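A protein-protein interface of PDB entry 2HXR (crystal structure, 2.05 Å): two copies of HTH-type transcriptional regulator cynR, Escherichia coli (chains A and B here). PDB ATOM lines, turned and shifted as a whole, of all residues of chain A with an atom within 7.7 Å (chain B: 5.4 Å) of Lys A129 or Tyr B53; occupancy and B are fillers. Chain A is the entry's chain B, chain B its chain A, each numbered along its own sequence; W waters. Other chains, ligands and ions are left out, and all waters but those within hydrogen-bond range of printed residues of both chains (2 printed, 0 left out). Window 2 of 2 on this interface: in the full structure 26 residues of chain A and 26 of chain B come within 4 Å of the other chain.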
ATOM      1  N   LEU A 106      14.243 -11.802  40.976  1.00  0.00           N
ATOM      2  CA  LEU A 106      14.291 -12.394  39.644  1.00  0.00           C
ATOM      3  C   LEU A 106      12.840 -12.328  39.197  1.00  0.00           C
ATOM      4  O   LEU A 106      11.979 -13.018  39.750  1.00  0.00           O
ATOM      5  CB  LEU A 106      14.744 -13.853  39.705  1.00  0.00           C
ATOM      6  CG  LEU A 106      14.858 -14.555  38.349  1.00  0.00           C
ATOM      7  CD1 LEU A 106      15.952 -13.877  37.524  1.00  0.00           C
ATOM      8  CD2 LEU A 106      15.189 -16.036  38.554  1.00  0.00           C
ATOM      9  N   HIS A 112       7.386 -19.439  33.613  1.00  0.00           N
ATOM     10  CA  HIS A 112       8.822 -19.663  33.785  1.00  0.00           C
ATOM     11  C   HIS A 112       9.049 -20.861  34.721  1.00  0.00           C
ATOM     12  O   HIS A 112       8.356 -21.026  35.721  1.00  0.00           O
ATOM     13  CB  HIS A 112       9.481 -18.403  34.361  1.00  0.00           C
ATOM     14  CG  HIS A 112      10.974 -18.490  34.471  1.00  0.00           C
ATOM     15  ND1 HIS A 112      11.609 -19.231  35.446  1.00  0.00           N
ATOM     16  CD2 HIS A 112      11.956 -17.933  33.722  1.00  0.00           C
ATOM     17  CE1 HIS A 112      12.918 -19.125  35.294  1.00  0.00           C
ATOM     18  NE2 HIS A 112      13.155 -18.343  34.255  1.00  0.00           N
ATOM     19  N   ARG A 124      21.209 -19.678  41.342  1.00  0.00           N
ATOM     20  CA  ARG A 124      20.319 -19.986  40.216  1.00  0.00           C
ATOM     21  C   ARG A 124      20.551 -19.053  39.036  1.00  0.00           C
ATOM     22  O   ARG A 124      20.325 -19.421  37.881  1.00  0.00           O
ATOM     23  CB  ARG A 124      18.859 -19.848  40.648  1.00  0.00           C
ATOM     24  CG  ARG A 124      18.375 -20.907  41.604  1.00  0.00           C
ATOM     25  CD  ARG A 124      18.137 -22.214  40.884  1.00  0.00           C
ATOM     26  NE  ARG A 124      17.329 -23.112  41.697  1.00  0.00           N
ATOM     27  CZ  ARG A 124      16.771 -24.226  41.241  1.00  0.00           C
ATOM     28  NH1 ARG A 124      16.938 -24.575  39.968  1.00  0.00           N
ATOM     29  NH2 ARG A 124      16.049 -24.988  42.057  1.00  0.00           N
ATOM     30  N   LEU A 125      20.969 -17.831  39.331  1.00  0.00           N
ATOM     31  CA  LEU A 125      21.221 -16.850  38.288  1.00  0.00           C
ATOM     32  C   LEU A 125      22.206 -17.335  37.232  1.00  0.00           C
ATOM     33  O   LEU A 125      22.139 -16.914  36.083  1.00  0.00           O
ATOM     34  CB  LEU A 125      21.743 -15.560  38.903  1.00  0.00           C
ATOM     35  CG  LEU A 125      20.683 -14.692  39.579  1.00  0.00           C
ATOM     36  CD1 LEU A 125      21.357 -13.598  40.390  1.00  0.00           C
ATOM     37  CD2 LEU A 125      19.767 -14.080  38.506  1.00  0.00           C
ATOM     38  N   HIS A 126      23.116 -18.219  37.624  1.00  0.00           N
ATOM     39  CA  HIS A 126      24.106 -18.718  36.685  1.00  0.00           C
ATOM     40  C   HIS A 126      23.470 -19.349  35.458  1.00  0.00           C
ATOM     41  O   HIS A 126      23.938 -19.141  34.338  1.00  0.00           O
ATOM     42  CB  HIS A 126      25.042 -19.728  37.379  1.00  0.00           C
ATOM     43  CG  HIS A 126      26.066 -20.320  36.465  1.00  0.00           C
ATOM     44  ND1 HIS A 126      25.758 -21.277  35.522  1.00  0.00           N
ATOM     45  CD2 HIS A 126      27.384 -20.048  36.306  1.00  0.00           C
ATOM     46  CE1 HIS A 126      26.840 -21.567  34.820  1.00  0.00           C
ATOM     47  NE2 HIS A 126      27.841 -20.834  35.277  1.00  0.00           N
ATOM     48  N   ASP A 127      22.392 -20.099  35.657  1.00  0.00           N
ATOM     49  CA  ASP A 127      21.727 -20.773  34.541  1.00  0.00           C
ATOM     50  C   ASP A 127      20.654 -19.933  33.856  1.00  0.00           C
ATOM     51  O   ASP A 127      20.060 -20.364  32.866  1.00  0.00           O
ATOM     52  CB  ASP A 127      21.102 -22.094  35.017  1.00  0.00           C
ATOM     53  CG  ASP A 127      22.123 -23.030  35.622  1.00  0.00           C
ATOM     54  OD1 ASP A 127      23.201 -23.172  35.009  1.00  0.00           O
ATOM     55  OD2 ASP A 127      21.854 -23.625  36.693  1.00  0.00           O
ATOM     56  N   GLU A 128      20.399 -18.740  34.378  1.00  0.00           N
ATOM     57  CA  GLU A 128      19.378 -17.879  33.782  1.00  0.00           C
ATOM     58  C   GLU A 128      19.865 -17.090  32.568  1.00  0.00           C
ATOM     59  O   GLU A 128      20.993 -16.590  32.550  1.00  0.00           O
ATOM     60  CB  GLU A 128      18.845 -16.881  34.816  1.00  0.00           C
ATOM     61  CG  GLU A 128      17.885 -17.458  35.844  1.00  0.00           C
ATOM     62  CD  GLU A 128      16.670 -18.090  35.199  1.00  0.00           C
ATOM     63  OE1 GLU A 128      15.990 -17.410  34.394  1.00  0.00           O
ATOM     64  OE2 GLU A 128      16.398 -19.267  35.500  1.00  0.00           O
ATOM     65  N   LYS A 129      19.007 -16.994  31.556  1.00  0.00           N
ATOM     66  CA  LYS A 129      19.297 -16.206  30.365  1.00  0.00           C
ATOM     67  C   LYS A 129      18.511 -14.940  30.683  1.00  0.00           C
ATOM     68  O   LYS A 129      17.284 -14.981  30.832  1.00  0.00           O
ATOM     69  CB  LYS A 129      18.761 -16.894  29.100  1.00  0.00           C
ATOM     70  CG  LYS A 129      19.556 -18.147  28.694  1.00  0.00           C
ATOM     71  CD  LYS A 129      19.036 -18.719  27.378  1.00  0.00           C
ATOM     72  CE  LYS A 129      19.803 -19.966  26.933  1.00  0.00           C
ATOM     73  NZ  LYS A 129      21.244 -19.705  26.614  1.00  0.00           N
ATOM     74  N   LEU A 130      19.214 -13.820  30.803  1.00  0.00           N
ATOM     75  CA  LEU A 130      18.575 -12.559  31.171  1.00  0.00           C
ATOM     76  C   LEU A 130      18.314 -11.490  30.113  1.00  0.00           C
ATOM     77  O   LEU A 130      19.010 -11.391  29.101  1.00  0.00           O
ATOM     78  CB  LEU A 130      19.386 -11.879  32.288  1.00  0.00           C
ATOM     79  CG  LEU A 130      19.735 -12.660  33.560  1.00  0.00           C
ATOM     80  CD1 LEU A 130      20.764 -11.885  34.380  1.00  0.00           C
ATOM     81  CD2 LEU A 130      18.464 -12.912  34.362  1.00  0.00           C
ATOM     82  N   VAL A 131      17.283 -10.691  30.392  1.00  0.00           N
ATOM     83  CA  VAL A 131      16.925  -9.536  29.595  1.00  0.00           C
ATOM     84  C   VAL A 131      17.158  -8.433  30.623  1.00  0.00           C
ATOM     85  O   VAL A 131      16.477  -8.372  31.645  1.00  0.00           O
ATOM     86  CB  VAL A 131      15.440  -9.508  29.186  1.00  0.00           C
ATOM     87  CG1 VAL A 131      15.091  -8.123  28.621  1.00  0.00           C
ATOM     88  CG2 VAL A 131      15.162 -10.567  28.145  1.00  0.00           C
ATOM     89  N   LEU A 132      18.124  -7.565  30.374  1.00  0.00           N
ATOM     90  CA  LEU A 132      18.422  -6.510  31.335  1.00  0.00           C
ATOM     91  C   LEU A 132      18.389  -5.105  30.776  1.00  0.00           C
ATOM     92  O   LEU A 132      18.409  -4.892  29.555  1.00  0.00           O
ATOM     93  CB  LEU A 132      19.811  -6.730  31.944  1.00  0.00           C
ATOM     94  CG  LEU A 132      20.010  -7.934  32.861  1.00  0.00           C
ATOM     95  CD1 LEU A 132      21.446  -7.961  33.355  1.00  0.00           C
ATOM     96  CD2 LEU A 132      19.032  -7.836  34.036  1.00  0.00           C
ATOM     97  N   PRO A 154      25.740 -14.436  34.855  1.00  0.00           N
ATOM     98  CA  PRO A 154      24.668 -14.950  34.006  1.00  0.00           C
ATOM     99  C   PRO A 154      24.732 -14.382  32.594  1.00  0.00           C
ATOM    100  O   PRO A 154      25.201 -13.271  32.364  1.00  0.00           O
ATOM    101  CB  PRO A 154      23.402 -14.519  34.749  1.00  0.00           C
ATOM    102  CG  PRO A 154      23.837 -13.246  35.442  1.00  0.00           C
ATOM    103  CD  PRO A 154      25.194 -13.636  35.968  1.00  0.00           C
ATOM    104  N   GLN A 155      24.255 -15.168  31.646  1.00  0.00           N
ATOM    105  CA  GLN A 155      24.229 -14.763  30.256  1.00  0.00           C
ATOM    106  C   GLN A 155      23.156 -13.690  30.037  1.00  0.00           C
ATOM    107  O   GLN A 155      22.017 -13.847  30.468  1.00  0.00           O
ATOM    108  CB  GLN A 155      23.931 -15.993  29.402  1.00  0.00           C
ATOM    109  CG  GLN A 155      24.003 -15.774  27.913  1.00  0.00           C
ATOM    110  CD  GLN A 155      23.779 -17.061  27.139  1.00  0.00           C
ATOM    111  OE1 GLN A 155      23.730 -17.054  25.912  1.00  0.00           O
ATOM    112  NE2 GLN A 155      23.643 -18.172  27.856  1.00  0.00           N
ATOM    113  N   VAL A 156      23.525 -12.589  29.396  1.00  0.00           N
ATOM    114  CA  VAL A 156      22.566 -11.531  29.089  1.00  0.00           C
ATOM    115  C   VAL A 156      22.315 -11.618  27.575  1.00  0.00           C
ATOM    116  O   VAL A 156      23.150 -11.196  26.774  1.00  0.00           O
ATOM    117  CB  VAL A 156      23.117 -10.135  29.446  1.00  0.00           C
ATOM    118  CG1 VAL A 156      22.120  -9.058  29.036  1.00  0.00           C
ATOM    119  CG2 VAL A 156      23.400 -10.048  30.949  1.00  0.00           C
ATOM    120  N   VAL A 157      21.170 -12.173  27.192  1.00  0.00           N
ATOM    121  CA  VAL A 157      20.846 -12.350  25.780  1.00  0.00           C
ATOM    122  C   VAL A 157      20.132 -11.170  25.142  1.00  0.00           C
ATOM    123  O   VAL A 157      20.107 -11.043  23.917  1.00  0.00           O
ATOM    124  CB  VAL A 157      20.009 -13.638  25.568  1.00  0.00           C
ATOM    125  CG1 VAL A 157      20.843 -14.859  25.964  1.00  0.00           C
ATOM    126  CG2 VAL A 157      18.743 -13.590  26.403  1.00  0.00           C
ATOM    127  N   ILE A 158      19.548 -10.305  25.965  1.00  0.00           N
ATOM    128  CA  ILE A 158      18.847  -9.132  25.446  1.00  0.00           C
ATOM    129  C   ILE A 158      19.018  -7.953  26.388  1.00  0.00           C
ATOM    130  O   ILE A 158      18.960  -8.104  27.609  1.00  0.00           O
ATOM    131  CB  ILE A 158      17.322  -9.378  25.289  1.00  0.00           C
ATOM    132  CG1 ILE A 158      17.066 -10.555  24.352  1.00  0.00           C
ATOM    133  CG2 ILE A 158      16.648  -8.126  24.733  1.00  0.00           C
ATOM    134  CD1 ILE A 158      15.607 -10.926  24.214  1.00  0.00           C
ATOM    135  N   LEU A 169       9.109  -8.354  27.095  1.00  0.00           N
ATOM    136  CA  LEU A 169       9.933  -9.471  26.649  1.00  0.00           C
ATOM    137  C   LEU A 169       9.826 -10.646  27.608  1.00  0.00           C
ATOM    138  O   LEU A 169       9.718 -11.799  27.172  1.00  0.00           O
ATOM    139  CB  LEU A 169      11.395  -9.021  26.497  1.00  0.00           C
ATOM    140  CG  LEU A 169      11.582  -8.017  25.348  1.00  0.00           C
ATOM    141  CD1 LEU A 169      12.955  -7.379  25.408  1.00  0.00           C
ATOM    142  CD2 LEU A 169      11.370  -8.726  24.014  1.00  0.00           C
ATOM    143  N   ILE A 170       9.841 -10.357  28.911  1.00  0.00           N
ATOM    144  CA  ILE A 170       9.736 -11.412  29.921  1.00  0.00           C
ATOM    145  C   ILE A 170       8.374 -12.111  29.855  1.00  0.00           C
ATOM    146  O   ILE A 170       8.295 -13.332  29.977  1.00  0.00           O
ATOM    147  CB  ILE A 170       9.936 -10.855  31.351  1.00  0.00           C
ATOM    148  CG1 ILE A 170      11.346 -10.277  31.501  1.00  0.00           C
ATOM    149  CG2 ILE A 170       9.664 -11.943  32.375  1.00  0.00           C
ATOM    150  CD1 ILE A 170      12.479 -11.250  31.185  1.00  0.00           C
ATOM    151  N   ARG A 172       6.456 -12.540  27.304  1.00  0.00           N
ATOM    152  CA  ARG A 172       6.368 -13.354  26.095  1.00  0.00           C
ATOM    153  C   ARG A 172       7.420 -14.427  25.857  1.00  0.00           C
ATOM    154  O   ARG A 172       7.387 -15.104  24.834  1.00  0.00           O
ATOM    155  CB  ARG A 172       6.321 -12.432  24.876  1.00  0.00           C
ATOM    156  CG  ARG A 172       5.112 -11.530  24.841  1.00  0.00           C
ATOM    157  CD  ARG A 172       5.163 -10.586  23.656  1.00  0.00           C
ATOM    158  NE  ARG A 172       4.029  -9.664  23.646  1.00  0.00           N
ATOM    159  CZ  ARG A 172       2.791  -9.987  23.278  1.00  0.00           C
ATOM    160  NH1 ARG A 172       2.511 -11.223  22.884  1.00  0.00           N
ATOM    161  NH2 ARG A 172       1.829  -9.069  23.300  1.00  0.00           N
ATOM    162  N   THR A 173       8.347 -14.602  26.788  1.00  0.00           N
ATOM    163  CA  THR A 173       9.392 -15.611  26.624  1.00  0.00           C
ATOM    164  C   THR A 173       9.585 -16.346  27.935  1.00  0.00           C
ATOM    165  O   THR A 173       8.810 -16.179  28.868  1.00  0.00           O
ATOM    166  CB  THR A 173      10.772 -14.981  26.268  1.00  0.00           C
ATOM    167  OG1 THR A 173      11.229 -14.183  27.375  1.00  0.00           O
ATOM    168  CG2 THR A 173      10.681 -14.120  25.013  1.00  0.00           C
ATOM    169  N   SER A 174      10.625 -17.166  27.999  1.00  0.00           N
ATOM    170  CA  SER A 174      10.937 -17.875  29.226  1.00  0.00           C
ATOM    171  C   SER A 174      12.214 -17.289  29.831  1.00  0.00           C
ATOM    172  O   SER A 174      12.899 -17.929  30.628  1.00  0.00           O
ATOM    173  CB  SER A 174      11.095 -19.372  28.963  1.00  0.00           C
ATOM    174  OG  SER A 174       9.820 -19.972  28.802  1.00  0.00           O
ATOM    175  N   LEU A 175      12.534 -16.061  29.443  1.00  0.00           N
ATOM    176  CA  LEU A 175      13.711 -15.395  29.979  1.00  0.00           C
ATOM    177  C   LEU A 175      13.348 -14.774  31.326  1.00  0.00           C
ATOM    178  O   LEU A 175      12.183 -14.773  31.735  1.00  0.00           O
ATOM    179  CB  LEU A 175      14.193 -14.307  29.017  1.00  0.00           C
ATOM    180  CG  LEU A 175      14.577 -14.837  27.624  1.00  0.00           C
ATOM    181  CD1 LEU A 175      14.932 -13.689  26.701  1.00  0.00           C
ATOM    182  CD2 LEU A 175      15.754 -15.818  27.759  1.00  0.00           C
ATOM    183  N   SER A 176      14.346 -14.258  32.024  1.00  0.00           N
ATOM    184  CA  SER A 176      14.094 -13.618  33.301  1.00  0.00           C
ATOM    185  C   SER A 176      14.851 -12.307  33.342  1.00  0.00           C
ATOM    186  O   SER A 176      15.724 -12.061  32.504  1.00  0.00           O
ATOM    187  CB  SER A 176      14.554 -14.513  34.450  1.00  0.00           C
ATOM    188  OG  SER A 176      15.936 -14.794  34.346  1.00  0.00           O
ATOM    189  N   THR A 177      14.490 -11.452  34.297  1.00  0.00           N
ATOM    190  CA  THR A 177      15.171 -10.189  34.475  1.00  0.00           C
ATOM    191  C   THR A 177      15.375  -9.944  35.970  1.00  0.00           C
ATOM    192  O   THR A 177      14.841 -10.678  36.813  1.00  0.00           O
ATOM    193  CB  THR A 177      14.378  -9.006  33.863  1.00  0.00           C
ATOM    194  OG1 THR A 177      15.181  -7.822  33.936  1.00  0.00           O
ATOM    195  CG2 THR A 177      13.067  -8.752  34.627  1.00  0.00           C
ATOM    196  N   LEU B  48       7.236  -8.652  18.433  1.00  0.00           N
ATOM    197  CA  LEU B  48       8.159  -8.979  17.354  1.00  0.00           C
ATOM    198  C   LEU B  48       9.493  -9.531  17.868  1.00  0.00           C
ATOM    199  O   LEU B  48       9.957 -10.574  17.408  1.00  0.00           O
ATOM    200  CB  LEU B  48       8.396  -7.744  16.486  1.00  0.00           C
ATOM    201  CG  LEU B  48       9.398  -7.899  15.338  1.00  0.00           C
ATOM    202  CD1 LEU B  48       9.085  -9.148  14.524  1.00  0.00           C
ATOM    203  CD2 LEU B  48       9.357  -6.645  14.475  1.00  0.00           C
ATOM    204  N   MET B  49      10.118  -8.841  18.814  1.00  0.00           N
ATOM    205  CA  MET B  49      11.382  -9.321  19.354  1.00  0.00           C
ATOM    206  C   MET B  49      11.224 -10.648  20.096  1.00  0.00           C
ATOM    207  O   MET B  49      12.091 -11.509  20.018  1.00  0.00           O
ATOM    208  CB  MET B  49      12.007  -8.266  20.269  1.00  0.00           C
ATOM    209  CG  MET B  49      12.630  -7.110  19.493  1.00  0.00           C
ATOM    210  SD  MET B  49      13.393  -5.721  20.612  1.00  0.00           S
ATOM    211  CE  MET B  49      14.768  -6.785  21.465  1.00  0.00           C
ATOM    212  N   ALA B  50      10.118 -10.816  20.810  1.00  0.00           N
ATOM    213  CA  ALA B  50       9.896 -12.057  21.537  1.00  0.00           C
ATOM    214  C   ALA B  50       9.820 -13.208  20.534  1.00  0.00           C
ATOM    215  O   ALA B  50      10.419 -14.261  20.749  1.00  0.00           O
ATOM    216  CB  ALA B  50       8.616 -11.974  22.353  1.00  0.00           C
ATOM    217  N   ASP B  51       9.088 -12.995  19.439  1.00  0.00           N
ATOM    218  CA  ASP B  51       8.959 -14.013  18.397  1.00  0.00           C
ATOM    219  C   ASP B  51      10.316 -14.318  17.762  1.00  0.00           C
ATOM    220  O   ASP B  51      10.685 -15.481  17.587  1.00  0.00           O
ATOM    221  CB  ASP B  51       7.981 -13.550  17.314  1.00  0.00           C
ATOM    222  CG  ASP B  51       6.547 -13.565  17.785  1.00  0.00           C
ATOM    223  OD1 ASP B  51       6.217 -14.397  18.660  1.00  0.00           O
ATOM    224  OD2 ASP B  51       5.742 -12.758  17.273  1.00  0.00           O
ATOM    225  N   PHE B  52      11.060 -13.268  17.424  1.00  0.00           N
ATOM    226  CA  PHE B  52      12.372 -13.437  16.821  1.00  0.00           C
ATOM    227  C   PHE B  52      13.278 -14.245  17.750  1.00  0.00           C
ATOM    228  O   PHE B  52      13.904 -15.229  17.333  1.00  0.00           O
ATOM    229  CB  PHE B  52      13.002 -12.069  16.528  1.00  0.00           C
ATOM    230  CG  PHE B  52      14.346 -12.148  15.840  1.00  0.00           C
ATOM    231  CD1 PHE B  52      15.512 -12.373  16.573  1.00  0.00           C
ATOM    232  CD2 PHE B  52      14.446 -11.990  14.456  1.00  0.00           C
ATOM    233  CE1 PHE B  52      16.764 -12.440  15.934  1.00  0.00           C
ATOM    234  CE2 PHE B  52      15.682 -12.054  13.807  1.00  0.00           C
ATOM    235  CZ  PHE B  52      16.844 -12.278  14.545  1.00  0.00           C
ATOM    236  N   TYR B  53      13.359 -13.830  19.011  1.00  0.00           N
ATOM    237  CA  TYR B  53      14.193 -14.551  19.971  1.00  0.00           C
ATOM    238  C   TYR B  53      13.803 -16.022  20.031  1.00  0.00           C
ATOM    239  O   TYR B  53      14.670 -16.892  20.052  1.00  0.00           O
ATOM    240  CB  TYR B  53      14.067 -13.975  21.383  1.00  0.00           C
ATOM    241  CG  TYR B  53      14.939 -14.712  22.376  1.00  0.00           C
ATOM    242  CD1 TYR B  53      16.307 -14.442  22.462  1.00  0.00           C
ATOM    243  CD2 TYR B  53      14.417 -15.724  23.177  1.00  0.00           C
ATOM    244  CE1 TYR B  53      17.135 -15.167  23.320  1.00  0.00           C
ATOM    245  CE2 TYR B  53      15.237 -16.459  24.041  1.00  0.00           C
ATOM    246  CZ  TYR B  53      16.593 -16.172  24.101  1.00  0.00           C
ATOM    247  OH  TYR B  53      17.413 -16.888  24.929  1.00  0.00           O
ATOM    248  N   ALA B  54      12.499 -16.289  20.091  1.00  0.00           N
ATOM    249  CA  ALA B  54      12.002 -17.666  20.163  1.00  0.00           C
ATOM    250  C   ALA B  54      12.476 -18.461  18.947  1.00  0.00           C
ATOM    251  O   ALA B  54      12.909 -19.600  19.075  1.00  0.00           O
ATOM    252  CB  ALA B  54      10.480 -17.674  20.233  1.00  0.00           C
ATOM    253  N   ARG B  55      12.399 -17.843  17.776  1.00  0.00           N
ATOM    254  CA  ARG B  55      12.836 -18.475  16.538  1.00  0.00           C
ATOM    255  C   ARG B  55      14.359 -18.585  16.445  1.00  0.00           C
ATOM    256  O   ARG B  55      14.887 -19.600  15.997  1.00  0.00           O
ATOM    257  CB  ARG B  55      12.314 -17.684  15.336  1.00  0.00           C
ATOM    258  CG  ARG B  55      10.801 -17.646  15.230  1.00  0.00           C
ATOM    259  CD  ARG B  55      10.365 -16.812  14.043  1.00  0.00           C
ATOM    260  NE  ARG B  55       8.924 -16.874  13.784  1.00  0.00           N
ATOM    261  CZ  ARG B  55       7.975 -16.511  14.646  1.00  0.00           C
ATOM    262  NH1 ARG B  55       8.291 -16.051  15.858  1.00  0.00           N
ATOM    263  NH2 ARG B  55       6.700 -16.596  14.287  1.00  0.00           N
ATOM    264  N   TYR B  56      15.069 -17.545  16.872  1.00  0.00           N
ATOM    265  CA  TYR B  56      16.533 -17.548  16.796  1.00  0.00           C
ATOM    266  C   TYR B  56      17.184 -17.201  18.130  1.00  0.00           C
ATOM    267  O   TYR B  56      17.752 -16.121  18.303  1.00  0.00           O
ATOM    268  CB  TYR B  56      16.974 -16.566  15.713  1.00  0.00           C
ATOM    269  CG  TYR B  56      16.288 -16.840  14.403  1.00  0.00           C
ATOM    270  CD1 TYR B  56      16.473 -18.058  13.740  1.00  0.00           C
ATOM    271  CD2 TYR B  56      15.435 -15.898  13.829  1.00  0.00           C
ATOM    272  CE1 TYR B  56      15.825 -18.331  12.531  1.00  0.00           C
ATOM    273  CE2 TYR B  56      14.783 -16.160  12.625  1.00  0.00           C
ATOM    274  CZ  TYR B  56      14.982 -17.379  11.983  1.00  0.00           C
ATOM    275  OH  TYR B  56      14.322 -17.647  10.808  1.00  0.00           O
ATOM    276  N   PRO B  57      17.123 -18.135  19.090  1.00  0.00           N
ATOM    277  CA  PRO B  57      17.670 -18.016  20.449  1.00  0.00           C
ATOM    278  C   PRO B  57      19.159 -17.685  20.547  1.00  0.00           C
ATOM    279  O   PRO B  57      19.599 -17.102  21.532  1.00  0.00           O
ATOM    280  CB  PRO B  57      17.379 -19.386  21.072  1.00  0.00           C
ATOM    281  CG  PRO B  57      16.272 -19.953  20.243  1.00  0.00           C
ATOM    282  CD  PRO B  57      16.590 -19.490  18.859  1.00  0.00           C
ATOM    283  N   ILE B  59      20.870 -15.572  18.819  1.00  0.00           N
ATOM    284  CA  ILE B  59      21.206 -14.199  18.473  1.00  0.00           C
ATOM    285  C   ILE B  59      20.970 -13.230  19.627  1.00  0.00           C
ATOM    286  O   ILE B  59      19.864 -13.139  20.165  1.00  0.00           O
ATOM    287  CB  ILE B  59      20.404 -13.741  17.239  1.00  0.00           C
ATOM    288  CG1 ILE B  59      20.658 -14.725  16.093  1.00  0.00           C
ATOM    289  CG2 ILE B  59      20.802 -12.314  16.846  1.00  0.00           C
ATOM    290  CD1 ILE B  59      19.939 -14.367  14.822  1.00  0.00           C
ATOM    291  N   LEU B  61      20.308  -9.787  21.290  1.00  0.00           N
ATOM    292  CA  LEU B  61      19.539  -8.618  20.881  1.00  0.00           C
ATOM    293  C   LEU B  61      19.746  -7.385  21.748  1.00  0.00           C
ATOM    294  O   LEU B  61      19.899  -7.480  22.973  1.00  0.00           O
ATOM    295  CB  LEU B  61      18.045  -8.945  20.892  1.00  0.00           C
ATOM    296  CG  LEU B  61      17.564 -10.136  20.070  1.00  0.00           C
ATOM    297  CD1 LEU B  61      16.037 -10.237  20.164  1.00  0.00           C
ATOM    298  CD2 LEU B  61      18.014  -9.952  18.619  1.00  0.00           C
HETATM  299  O   HOH W   1      19.740 -17.826  24.243  1.00  0.00           O
HETATM  300  O   HOH W   2       5.105 -12.731  21.284  1.00  0.00           O
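Water W1 lies within hydrogen-bond range of the side-chain hydroxyl of Tyr B53 (2.6 Å), the backbone carbonyl oxygen of Pro B57 (2.8 Å) and the side-chain amino group of Lys A129 (3.4 Å).
Water W2 bridges OD1 of Asp B51 (3.3 Å) and NH1 of Arg A172 (3.4 Å).
No position is printed for both chains.
Of the 9 pairs that touch across the chains among the printed residues, none has its exchanged pair printed and touching as well.
O of Val A157 is in hydrogen-bond range of N of Leu B61 (2.9 Å).
Lys A129 touches Tyr B53.
CG2 of Val A157 touches CE1 of Tyr B53, at 3.8 Å.
Ile A158 touches Tyr B53 (CD1 to CD1, 3.99 Å).
Ile A158 touches Leu B61.
Leu A169 touches Met B49.
Arg A172 touches Ala B50 (CB to CB, 3.4 Å).
Ala B50 touches Thr A173.
Leu A175 touches Tyr B53 (CD2 to OH, 3.5 Å).
Lys A129 touches one residue of chain B.
Of the printed residues of chain A, Tyr B53 touches Lys A129 (3.5 Å), Val A157 (3.8 Å), Ile A158 (3.99 Å) and Leu A175 (3.5 Å).
Printed residues of chain A within 4 Å of Met B49: Leu A169 (3.8 Å).
Printed residues of chain A within 4 Å of Ala B50: Arg A172 (3.4 Å) and Thr A173 (3.99 Å).
Of the printed residues of chain B, Ile A158 touches Tyr B53 and Leu B61.
Of the printed residues of chain B, Leu A175 touches Tyr B53.
Ser A176 touches none of the printed residues of chain B.
Val A156 touches none of the printed residues of chain B.
The nearest printed residue of chain B that does not touch Leu A169 is Ala B50 (4.03 Å).
The backbone NH of Val A157 is in hydrogen-bond range of the backbone carbonyl oxygen of Leu A130, at 3.0 Å.
O of Leu A130 sits at hydrogen-bond distance from N of Ile A158.
OG1 of Thr A173 is in hydrogen-bond range of O of Leu A169.
N of Leu A175 lies within hydrogen-bond range of OG1 of Thr A173, at 3.1 Å.
O of Lys A129 lies within hydrogen-bond range of N of Ser A176 (3.3 Å).
The backbone NH of Leu A132 sits at hydrogen-bond distance from the backbone carbonyl oxygen of Ile A158 (2.9 Å).
Along chain B the printed residues that touch a printed residue of chain A span positions 49 to 61.
Of the 24 printed residues of chain A, 7 touch a printed residue of chain B.
Hydrophobic or aromatic side chains of chain A that line the printed part of chain B: Val A157, Ile A158, Leu A169 and Leu A175.
Along chain A the printed residues that touch a printed residue of chain B span positions 129 to 175.
Among the printed residues, no Asp or Glu carboxylate lies within 4 Å of a Lys or Arg side-chain nitrogen of the other chain.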
